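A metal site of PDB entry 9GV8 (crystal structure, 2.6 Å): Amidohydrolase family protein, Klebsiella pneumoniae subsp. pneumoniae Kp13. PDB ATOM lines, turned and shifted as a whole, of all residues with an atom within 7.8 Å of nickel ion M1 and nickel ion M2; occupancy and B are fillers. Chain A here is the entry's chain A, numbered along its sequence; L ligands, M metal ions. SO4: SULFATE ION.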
ATOM      1  N   HIS A  62     -24.250   0.386  10.530  1.00  0.00           N
ATOM      2  CA  HIS A  62     -24.738  -0.988  10.391  1.00  0.00           C
ATOM      3  C   HIS A  62     -25.571  -1.076   9.113  1.00  0.00           C
ATOM      4  O   HIS A  62     -26.768  -0.768   9.118  1.00  0.00           O
ATOM      5  CB  HIS A  62     -25.547  -1.414  11.605  1.00  0.00           C
ATOM      6  CG  HIS A  62     -25.776  -2.889  11.698  1.00  0.00           C
ATOM      7  ND1 HIS A  62     -25.086  -3.704  12.571  1.00  0.00           N
ATOM      8  CD2 HIS A  62     -26.595  -3.705  11.002  1.00  0.00           C
ATOM      9  CE1 HIS A  62     -25.484  -4.951  12.422  1.00  0.00           C
ATOM     10  NE2 HIS A  62     -26.400  -4.985  11.477  1.00  0.00           N
ATOM     11  N   THR A  63     -24.937  -1.489   8.019  1.00  0.00           N
ATOM     12  CA  THR A  63     -25.601  -1.685   6.737  1.00  0.00           C
ATOM     13  C   THR A  63     -25.256  -3.070   6.194  1.00  0.00           C
ATOM     14  O   THR A  63     -24.324  -3.736   6.656  1.00  0.00           O
ATOM     15  CB  THR A  63     -25.204  -0.619   5.709  1.00  0.00           C
ATOM     16  OG1 THR A  63     -23.841  -0.827   5.310  1.00  0.00           O
ATOM     17  CG2 THR A  63     -25.339   0.763   6.297  1.00  0.00           C
ATOM     18  N   HIS A  64     -26.032  -3.488   5.204  1.00  0.00           N
ATOM     19  CA  HIS A  64     -25.743  -4.670   4.398  1.00  0.00           C
ATOM     20  C   HIS A  64     -25.681  -4.292   2.923  1.00  0.00           C
ATOM     21  O   HIS A  64     -26.130  -5.027   2.038  1.00  0.00           O
ATOM     22  CB  HIS A  64     -26.776  -5.769   4.641  1.00  0.00           C
ATOM     23  CG  HIS A  64     -26.741  -6.337   6.020  1.00  0.00           C
ATOM     24  ND1 HIS A  64     -25.806  -7.268   6.413  1.00  0.00           N
ATOM     25  CD2 HIS A  64     -27.526  -6.116   7.101  1.00  0.00           C
ATOM     26  CE1 HIS A  64     -26.005  -7.599   7.676  1.00  0.00           C
ATOM     27  NE2 HIS A  64     -27.052  -6.914   8.118  1.00  0.00           N
ATOM     28  N   GLY A  89     -20.646  -4.930   5.534  1.00  0.00           N
ATOM     29  CA  GLY A  89     -19.983  -6.118   6.028  1.00  0.00           C
ATOM     30  C   GLY A  89     -20.265  -6.434   7.476  1.00  0.00           C
ATOM     31  O   GLY A  89     -19.352  -6.855   8.208  1.00  0.00           O
ATOM     32  N   ASN A  90     -21.507  -6.264   7.925  1.00  0.00           N
ATOM     33  CA  ASN A  90     -21.873  -6.526   9.304  1.00  0.00           C
ATOM     34  C   ASN A  90     -22.429  -7.941   9.472  1.00  0.00           C
ATOM     35  O   ASN A  90     -22.753  -8.619   8.494  1.00  0.00           O
ATOM     36  CB  ASN A  90     -22.900  -5.507   9.795  1.00  0.00           C
ATOM     37  CG  ASN A  90     -22.338  -4.112   9.909  1.00  0.00           C
ATOM     38  OD1 ASN A  90     -21.802  -3.721  10.943  1.00  0.00           O
ATOM     39  ND2 ASN A  90     -22.447  -3.343   8.827  1.00  0.00           N
ATOM     40  N   CYS A  91     -22.523  -8.366  10.727  1.00  0.00           N
ATOM     41  CA  CYS A  91     -23.167  -9.623  11.113  1.00  0.00           C
ATOM     42  C   CYS A  91     -22.460 -10.830  10.508  1.00  0.00           C
ATOM     43  O   CYS A  91     -23.084 -11.830  10.143  1.00  0.00           O
ATOM     44  CB  CYS A  91     -24.647  -9.616  10.730  1.00  0.00           C
ATOM     45  SG  CYS A  91     -25.546  -8.198  11.403  1.00  0.00           S
ATOM     46  N   GLY A  92     -21.135 -10.741  10.396  1.00  0.00           N
ATOM     47  CA  GLY A  92     -20.336 -11.845   9.913  1.00  0.00           C
ATOM     48  C   GLY A  92     -20.415 -12.108   8.433  1.00  0.00           C
ATOM     49  O   GLY A  92     -19.719 -13.011   7.946  1.00  0.00           O
ATOM     50  N   ILE A  93     -21.219 -11.349   7.685  1.00  0.00           N
ATOM     51  CA  ILE A  93     -21.350 -11.521   6.248  1.00  0.00           C
ATOM     52  C   ILE A  93     -20.800 -10.279   5.565  1.00  0.00           C
ATOM     53  O   ILE A  93     -21.127  -9.142   5.959  1.00  0.00           O
ATOM     54  CB  ILE A  93     -22.809 -11.771   5.846  1.00  0.00           C
ATOM     55  CG1 ILE A  93     -23.729 -10.715   6.463  1.00  0.00           C
ATOM     56  CG2 ILE A  93     -23.255 -13.158   6.292  1.00  0.00           C
ATOM     57  CD1 ILE A  93     -25.147 -10.761   5.945  1.00  0.00           C
ATOM     58  N   PRO A 107     -26.201 -16.331   6.454  1.00  0.00           N
ATOM     59  CA  PRO A 107     -27.071 -15.418   5.716  1.00  0.00           C
ATOM     60  C   PRO A 107     -26.351 -14.581   4.659  1.00  0.00           C
ATOM     61  O   PRO A 107     -26.725 -13.439   4.437  1.00  0.00           O
ATOM     62  CB  PRO A 107     -27.621 -14.528   6.826  1.00  0.00           C
ATOM     63  CG  PRO A 107     -26.429 -14.371   7.745  1.00  0.00           C
ATOM     64  CD  PRO A 107     -25.670 -15.678   7.669  1.00  0.00           C
ATOM     65  N   LEU A 110     -28.203 -12.527   1.791  1.00  0.00           N
ATOM     66  CA  LEU A 110     -28.785 -11.198   1.918  1.00  0.00           C
ATOM     67  C   LEU A 110     -28.049 -10.186   1.046  1.00  0.00           C
ATOM     68  O   LEU A 110     -28.662  -9.230   0.555  1.00  0.00           O
ATOM     69  CB  LEU A 110     -28.752 -10.740   3.377  1.00  0.00           C
ATOM     70  CG  LEU A 110     -29.479 -11.584   4.434  1.00  0.00           C
ATOM     71  CD1 LEU A 110     -29.366 -10.937   5.810  1.00  0.00           C
ATOM     72  CD2 LEU A 110     -30.939 -11.805   4.070  1.00  0.00           C
ATOM     73  N   THR A 184     -19.182 -10.394  13.316  1.00  0.00           N
ATOM     74  CA  THR A 184     -19.604 -11.769  13.542  1.00  0.00           C
ATOM     75  C   THR A 184     -21.124 -11.842  13.610  1.00  0.00           C
ATOM     76  O   THR A 184     -21.786 -10.900  14.059  1.00  0.00           O
ATOM     77  CB  THR A 184     -19.002 -12.355  14.831  1.00  0.00           C
ATOM     78  OG1 THR A 184     -19.367 -11.532  15.947  1.00  0.00           O
ATOM     79  CG2 THR A 184     -17.486 -12.432  14.728  1.00  0.00           C
ATOM     80  N   GLY A 185     -21.653 -12.967  13.157  1.00  0.00           N
ATOM     81  CA  GLY A 185     -23.065 -13.282  13.302  1.00  0.00           C
ATOM     82  C   GLY A 185     -23.223 -14.661  13.898  1.00  0.00           C
ATOM     83  O   GLY A 185     -23.512 -15.625  13.184  1.00  0.00           O
ATOM     84  N   LEU A 186     -23.028 -14.763  15.209  1.00  0.00           N
ATOM     85  CA  LEU A 186     -22.891 -16.076  15.843  1.00  0.00           C
ATOM     86  C   LEU A 186     -24.214 -16.820  15.911  1.00  0.00           C
ATOM     87  O   LEU A 186     -24.219 -18.062  15.940  1.00  0.00           O
ATOM     88  CB  LEU A 186     -22.288 -15.920  17.233  1.00  0.00           C
ATOM     89  CG  LEU A 186     -20.946 -15.187  17.287  1.00  0.00           C
ATOM     90  CD1 LEU A 186     -20.600 -14.837  18.721  1.00  0.00           C
ATOM     91  CD2 LEU A 186     -19.850 -16.032  16.654  1.00  0.00           C
ATOM     92  N   ALA A 187     -25.336 -16.106  15.956  1.00  0.00           N
ATOM     93  CA  ALA A 187     -26.640 -16.766  16.052  1.00  0.00           C
ATOM     94  C   ALA A 187     -26.978 -17.587  14.817  1.00  0.00           C
ATOM     95  O   ALA A 187     -27.830 -18.473  14.894  1.00  0.00           O
ATOM     96  CB  ALA A 187     -27.741 -15.728  16.306  1.00  0.00           C
ATOM     97  N   TYR A 188     -26.324 -17.322  13.688  1.00  0.00           N
ATOM     98  CA  TYR A 188     -26.599 -18.062  12.465  1.00  0.00           C
ATOM     99  C   TYR A 188     -25.893 -19.404  12.477  1.00  0.00           C
ATOM    100  O   TYR A 188     -24.820 -19.574  13.079  1.00  0.00           O
ATOM    101  CB  TYR A 188     -26.175 -17.239  11.247  1.00  0.00           C
ATOM    102  CG  TYR A 188     -26.962 -15.950  11.112  1.00  0.00           C
ATOM    103  CD1 TYR A 188     -28.197 -15.945  10.474  1.00  0.00           C
ATOM    104  CD2 TYR A 188     -26.490 -14.761  11.629  1.00  0.00           C
ATOM    105  CE1 TYR A 188     -28.925 -14.790  10.348  1.00  0.00           C
ATOM    106  CE2 TYR A 188     -27.217 -13.591  11.502  1.00  0.00           C
ATOM    107  CZ  TYR A 188     -28.432 -13.610  10.857  1.00  0.00           C
ATOM    108  OH  TYR A 188     -29.161 -12.453  10.740  1.00  0.00           O
ATOM    109  N   THR A 215     -20.281  -7.282  16.728  1.00  0.00           N
ATOM    110  CA  THR A 215     -20.813  -8.633  16.925  1.00  0.00           C
ATOM    111  C   THR A 215     -22.326  -8.633  16.891  1.00  0.00           C
ATOM    112  O   THR A 215     -22.980  -7.867  17.617  1.00  0.00           O
ATOM    113  CB  THR A 215     -20.321  -9.230  18.247  1.00  0.00           C
ATOM    114  OG1 THR A 215     -21.066 -10.425  18.534  1.00  0.00           O
ATOM    115  CG2 THR A 215     -20.482  -8.247  19.401  1.00  0.00           C
ATOM    116  N   HIS A 216     -22.886  -9.484  16.033  1.00  0.00           N
ATOM    117  CA  HIS A 216     -24.244  -9.974  16.199  1.00  0.00           C
ATOM    118  C   HIS A 216     -24.183 -11.074  17.250  1.00  0.00           C
ATOM    119  O   HIS A 216     -23.596 -12.137  17.002  1.00  0.00           O
ATOM    120  CB  HIS A 216     -24.796 -10.473  14.866  1.00  0.00           C
ATOM    121  CG  HIS A 216     -26.199 -10.997  14.930  1.00  0.00           C
ATOM    122  ND1 HIS A 216     -27.118 -10.777  13.935  1.00  0.00           N
ATOM    123  CD2 HIS A 216     -26.839 -11.753  15.869  1.00  0.00           C
ATOM    124  CE1 HIS A 216     -28.266 -11.351  14.249  1.00  0.00           C
ATOM    125  NE2 HIS A 216     -28.119 -11.951  15.417  1.00  0.00           N
ATOM    126  N   LEU A 217     -24.764 -10.819  18.413  1.00  0.00           N
ATOM    127  CA  LEU A 217     -24.592 -11.712  19.564  1.00  0.00           C
ATOM    128  C   LEU A 217     -25.070 -13.122  19.236  1.00  0.00           C
ATOM    129  O   LEU A 217     -25.922 -13.330  18.373  1.00  0.00           O
ATOM    130  CB  LEU A 217     -25.344 -11.163  20.775  1.00  0.00           C
ATOM    131  CG  LEU A 217     -24.817  -9.856  21.371  1.00  0.00           C
ATOM    132  CD1 LEU A 217     -25.730  -9.373  22.482  1.00  0.00           C
ATOM    133  CD2 LEU A 217     -23.404 -10.037  21.888  1.00  0.00           C
ATOM    134  N   GLU A 220     -29.847 -13.094  21.151  1.00  0.00           N
ATOM    135  CA  GLU A 220     -30.450 -11.832  21.571  1.00  0.00           C
ATOM    136  C   GLU A 220     -31.774 -12.058  22.281  1.00  0.00           C
ATOM    137  O   GLU A 220     -32.726 -11.289  22.114  1.00  0.00           O
ATOM    138  CB  GLU A 220     -30.629 -10.897  20.378  1.00  0.00           C
ATOM    139  CG  GLU A 220     -29.335 -10.286  19.861  1.00  0.00           C
ATOM    140  CD  GLU A 220     -29.573  -8.989  19.121  1.00  0.00           C
ATOM    141  OE1 GLU A 220     -30.275  -9.009  18.090  1.00  0.00           O
ATOM    142  OE2 GLU A 220     -29.051  -7.948  19.567  1.00  0.00           O
ATOM    143  N   SER A 245     -23.757  -5.115  17.926  1.00  0.00           N
ATOM    144  CA  SER A 245     -24.616  -4.727  16.807  1.00  0.00           C
ATOM    145  C   SER A 245     -26.088  -4.901  17.164  1.00  0.00           C
ATOM    146  O   SER A 245     -26.465  -5.808  17.916  1.00  0.00           O
ATOM    147  CB  SER A 245     -24.287  -5.565  15.569  1.00  0.00           C
ATOM    148  OG  SER A 245     -22.967  -5.330  15.130  1.00  0.00           O
ATOM    149  N   HIS A 246     -26.929  -4.028  16.579  1.00  0.00           N
ATOM    150  CA  HIS A 246     -28.367  -3.926  16.807  1.00  0.00           C
ATOM    151  C   HIS A 246     -28.812  -4.465  18.152  1.00  0.00           C
ATOM    152  O   HIS A 246     -29.578  -5.438  18.217  1.00  0.00           O
ATOM    153  CB  HIS A 246     -29.137  -4.625  15.678  1.00  0.00           C
ATOM    154  CG  HIS A 246     -28.630  -5.996  15.366  1.00  0.00           C
ATOM    155  ND1 HIS A 246     -28.378  -6.931  16.343  1.00  0.00           N
ATOM    156  CD2 HIS A 246     -28.326  -6.589  14.187  1.00  0.00           C
ATOM    157  CE1 HIS A 246     -27.936  -8.041  15.776  1.00  0.00           C
ATOM    158  NE2 HIS A 246     -27.904  -7.868  14.467  1.00  0.00           N
ATOM    159  N   LYS A 248     -30.781  -5.315  21.199  1.00  0.00           N
ATOM    160  CA  LYS A 248     -32.218  -5.369  21.412  1.00  0.00           C
ATOM    161  C   LYS A 248     -32.516  -6.489  22.399  1.00  0.00           C
ATOM    162  O   LYS A 248     -31.742  -7.435  22.551  1.00  0.00           O
ATOM    163  CB  LYS A 248     -32.967  -5.602  20.086  1.00  0.00           C
ATOM    164  CG  LYS A 248     -32.793  -7.000  19.521  1.00  0.00           C
ATOM    165  CD  LYS A 248     -33.297  -7.116  18.096  1.00  0.00           C
ATOM    166  CE  LYS A 248     -32.424  -6.325  17.132  1.00  0.00           C
ATOM    167  NZ  LYS A 248     -32.681  -6.690  15.715  1.00  0.00           N
ATOM    168  N   ASP A 277     -24.827  -0.211  18.710  1.00  0.00           N
ATOM    169  CA  ASP A 277     -25.707   0.535  17.827  1.00  0.00           C
ATOM    170  C   ASP A 277     -27.090  -0.106  17.857  1.00  0.00           C
ATOM    171  O   ASP A 277     -27.275  -1.216  18.370  1.00  0.00           O
ATOM    172  CB  ASP A 277     -25.170   0.595  16.387  1.00  0.00           C
ATOM    173  CG  ASP A 277     -25.100  -0.769  15.734  1.00  0.00           C
ATOM    174  OD1 ASP A 277     -24.048  -1.422  15.833  1.00  0.00           O
ATOM    175  OD2 ASP A 277     -26.119  -1.194  15.138  1.00  0.00           O
ATOM    176  N   SER A 361     -29.094   1.998  10.783  1.00  0.00           N
ATOM    177  CA  SER A 361     -30.384   1.711  10.163  1.00  0.00           C
ATOM    178  C   SER A 361     -30.652   0.212  10.084  1.00  0.00           C
ATOM    179  O   SER A 361     -31.759  -0.239  10.366  1.00  0.00           O
ATOM    180  CB  SER A 361     -30.455   2.338   8.769  1.00  0.00           C
ATOM    181  OG  SER A 361     -29.563   1.702   7.873  1.00  0.00           O
ATOM    182  N   ASP A 362     -29.633  -0.567   9.714  1.00  0.00           N
ATOM    183  CA  ASP A 362     -29.783  -1.998   9.449  1.00  0.00           C
ATOM    184  C   ASP A 362     -30.880  -2.217   8.419  1.00  0.00           C
ATOM    185  O   ASP A 362     -31.777  -3.054   8.580  1.00  0.00           O
ATOM    186  CB  ASP A 362     -30.052  -2.776  10.735  1.00  0.00           C
ATOM    187  CG  ASP A 362     -29.908  -4.279  10.554  1.00  0.00           C
ATOM    188  OD1 ASP A 362     -29.531  -4.713   9.444  1.00  0.00           O
ATOM    189  OD2 ASP A 362     -30.185  -5.018  11.517  1.00  0.00           O
ATOM    190  N   GLY A 363     -30.812  -1.442   7.339  1.00  0.00           N
ATOM    191  CA  GLY A 363     -31.798  -1.544   6.292  1.00  0.00           C
ATOM    192  C   GLY A 363     -31.509  -2.689   5.334  1.00  0.00           C
ATOM    193  O   GLY A 363     -30.368  -3.043   5.076  1.00  0.00           O
ATOM    194  N   LEU A 364     -32.582  -3.270   4.811  1.00  0.00           N
ATOM    195  CA  LEU A 364     -32.510  -4.408   3.909  1.00  0.00           C
ATOM    196  C   LEU A 364     -32.975  -3.965   2.524  1.00  0.00           C
ATOM    197  O   LEU A 364     -34.187  -3.971   2.250  1.00  0.00           O
ATOM    198  CB  LEU A 364     -33.354  -5.572   4.418  1.00  0.00           C
ATOM    199  CG  LEU A 364     -32.892  -6.470   5.589  1.00  0.00           C
ATOM    200  CD1 LEU A 364     -31.671  -7.304   5.205  1.00  0.00           C
ATOM    201  CD2 LEU A 364     -32.631  -5.683   6.870  1.00  0.00           C
ATOM    202  N   ARG A 373     -37.076   1.479   8.254  1.00  0.00           N
ATOM    203  CA  ARG A 373     -35.775   1.979   8.685  1.00  0.00           C
ATOM    204  C   ARG A 373     -34.842   2.225   7.506  1.00  0.00           C
ATOM    205  O   ARG A 373     -33.886   3.009   7.642  1.00  0.00           O
ATOM    206  CB  ARG A 373     -35.135   1.002   9.661  1.00  0.00           C
ATOM    207  CG  ARG A 373     -34.799  -0.356   9.066  1.00  0.00           C
ATOM    208  CD  ARG A 373     -34.679  -1.403  10.160  1.00  0.00           C
ATOM    209  NE  ARG A 373     -34.342  -2.716   9.613  1.00  0.00           N
ATOM    210  CZ  ARG A 373     -34.413  -3.844  10.305  1.00  0.00           C
ATOM    211  NH1 ARG A 373     -34.812  -3.858  11.562  1.00  0.00           N
ATOM    212  NH2 ARG A 373     -34.065  -4.982   9.722  1.00  0.00           N
HETATM  213  S   SO4 L   1     -29.463  -9.075  10.465  1.00  0.00           S
HETATM  214  O1  SO4 L   1     -30.923  -9.318  10.283  1.00  0.00           O
HETATM  215  O2  SO4 L   1     -28.684  -9.868   9.467  1.00  0.00           O
HETATM  216  O3  SO4 L   1     -29.179  -7.615  10.286  1.00  0.00           O
HETATM  217  O4  SO4 L   1     -29.052  -9.485  11.854  1.00  0.00           O
HETATM  218 NI    NI M   1     -27.080  -6.642  10.212  1.00  0.00          NI
HETATM  219 NI    NI M   2     -27.391  -9.015  12.783  1.00  0.00          NI
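A ring nitrogen (ND1) of His 246 sits at hydrogen-bond distance from the side-chain carboxylate (OE1) of Glu 220, 3.3 Å away. The side-chain carboxylate of Asp 277 is in hydrogen-bond range of the backbone NH of His 246 (3.3 Å). N of His 216 lies within hydrogen-bond range of O of Thr 184 (2.7 Å). N of Leu 186 sits at hydrogen-bond distance from O of His 216 (3.2 Å). O of His 62 sits at hydrogen-bond distance from N of Asp 362. NE of Arg 373 is in hydrogen-bond range of O of Asp 362 (2.8 Å).
OD1 of Asp 362 touches nickel ion M1, 3.2 Å away.
Of the 28 residues printed, 3 come within 4 Å of nickel ion M2. The nearest printed residue that does not touch nickel ion M2 is His 62 (4.4 Å).
Nickel ion M1 is bound by NE2 of His 64 (2.1 Å), NE2 of His 62 (2.2 Å), O3 of the ligand (2.3 Å) and SG of Cys 91 (2.5 Å).
Nickel ion M2 is bound by O4 of the ligand (2.0 Å), NE2 of His 246 (2.1 Å), ND1 of His 216 (2.1 Å) and SG of Cys 91 (2.4 Å).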
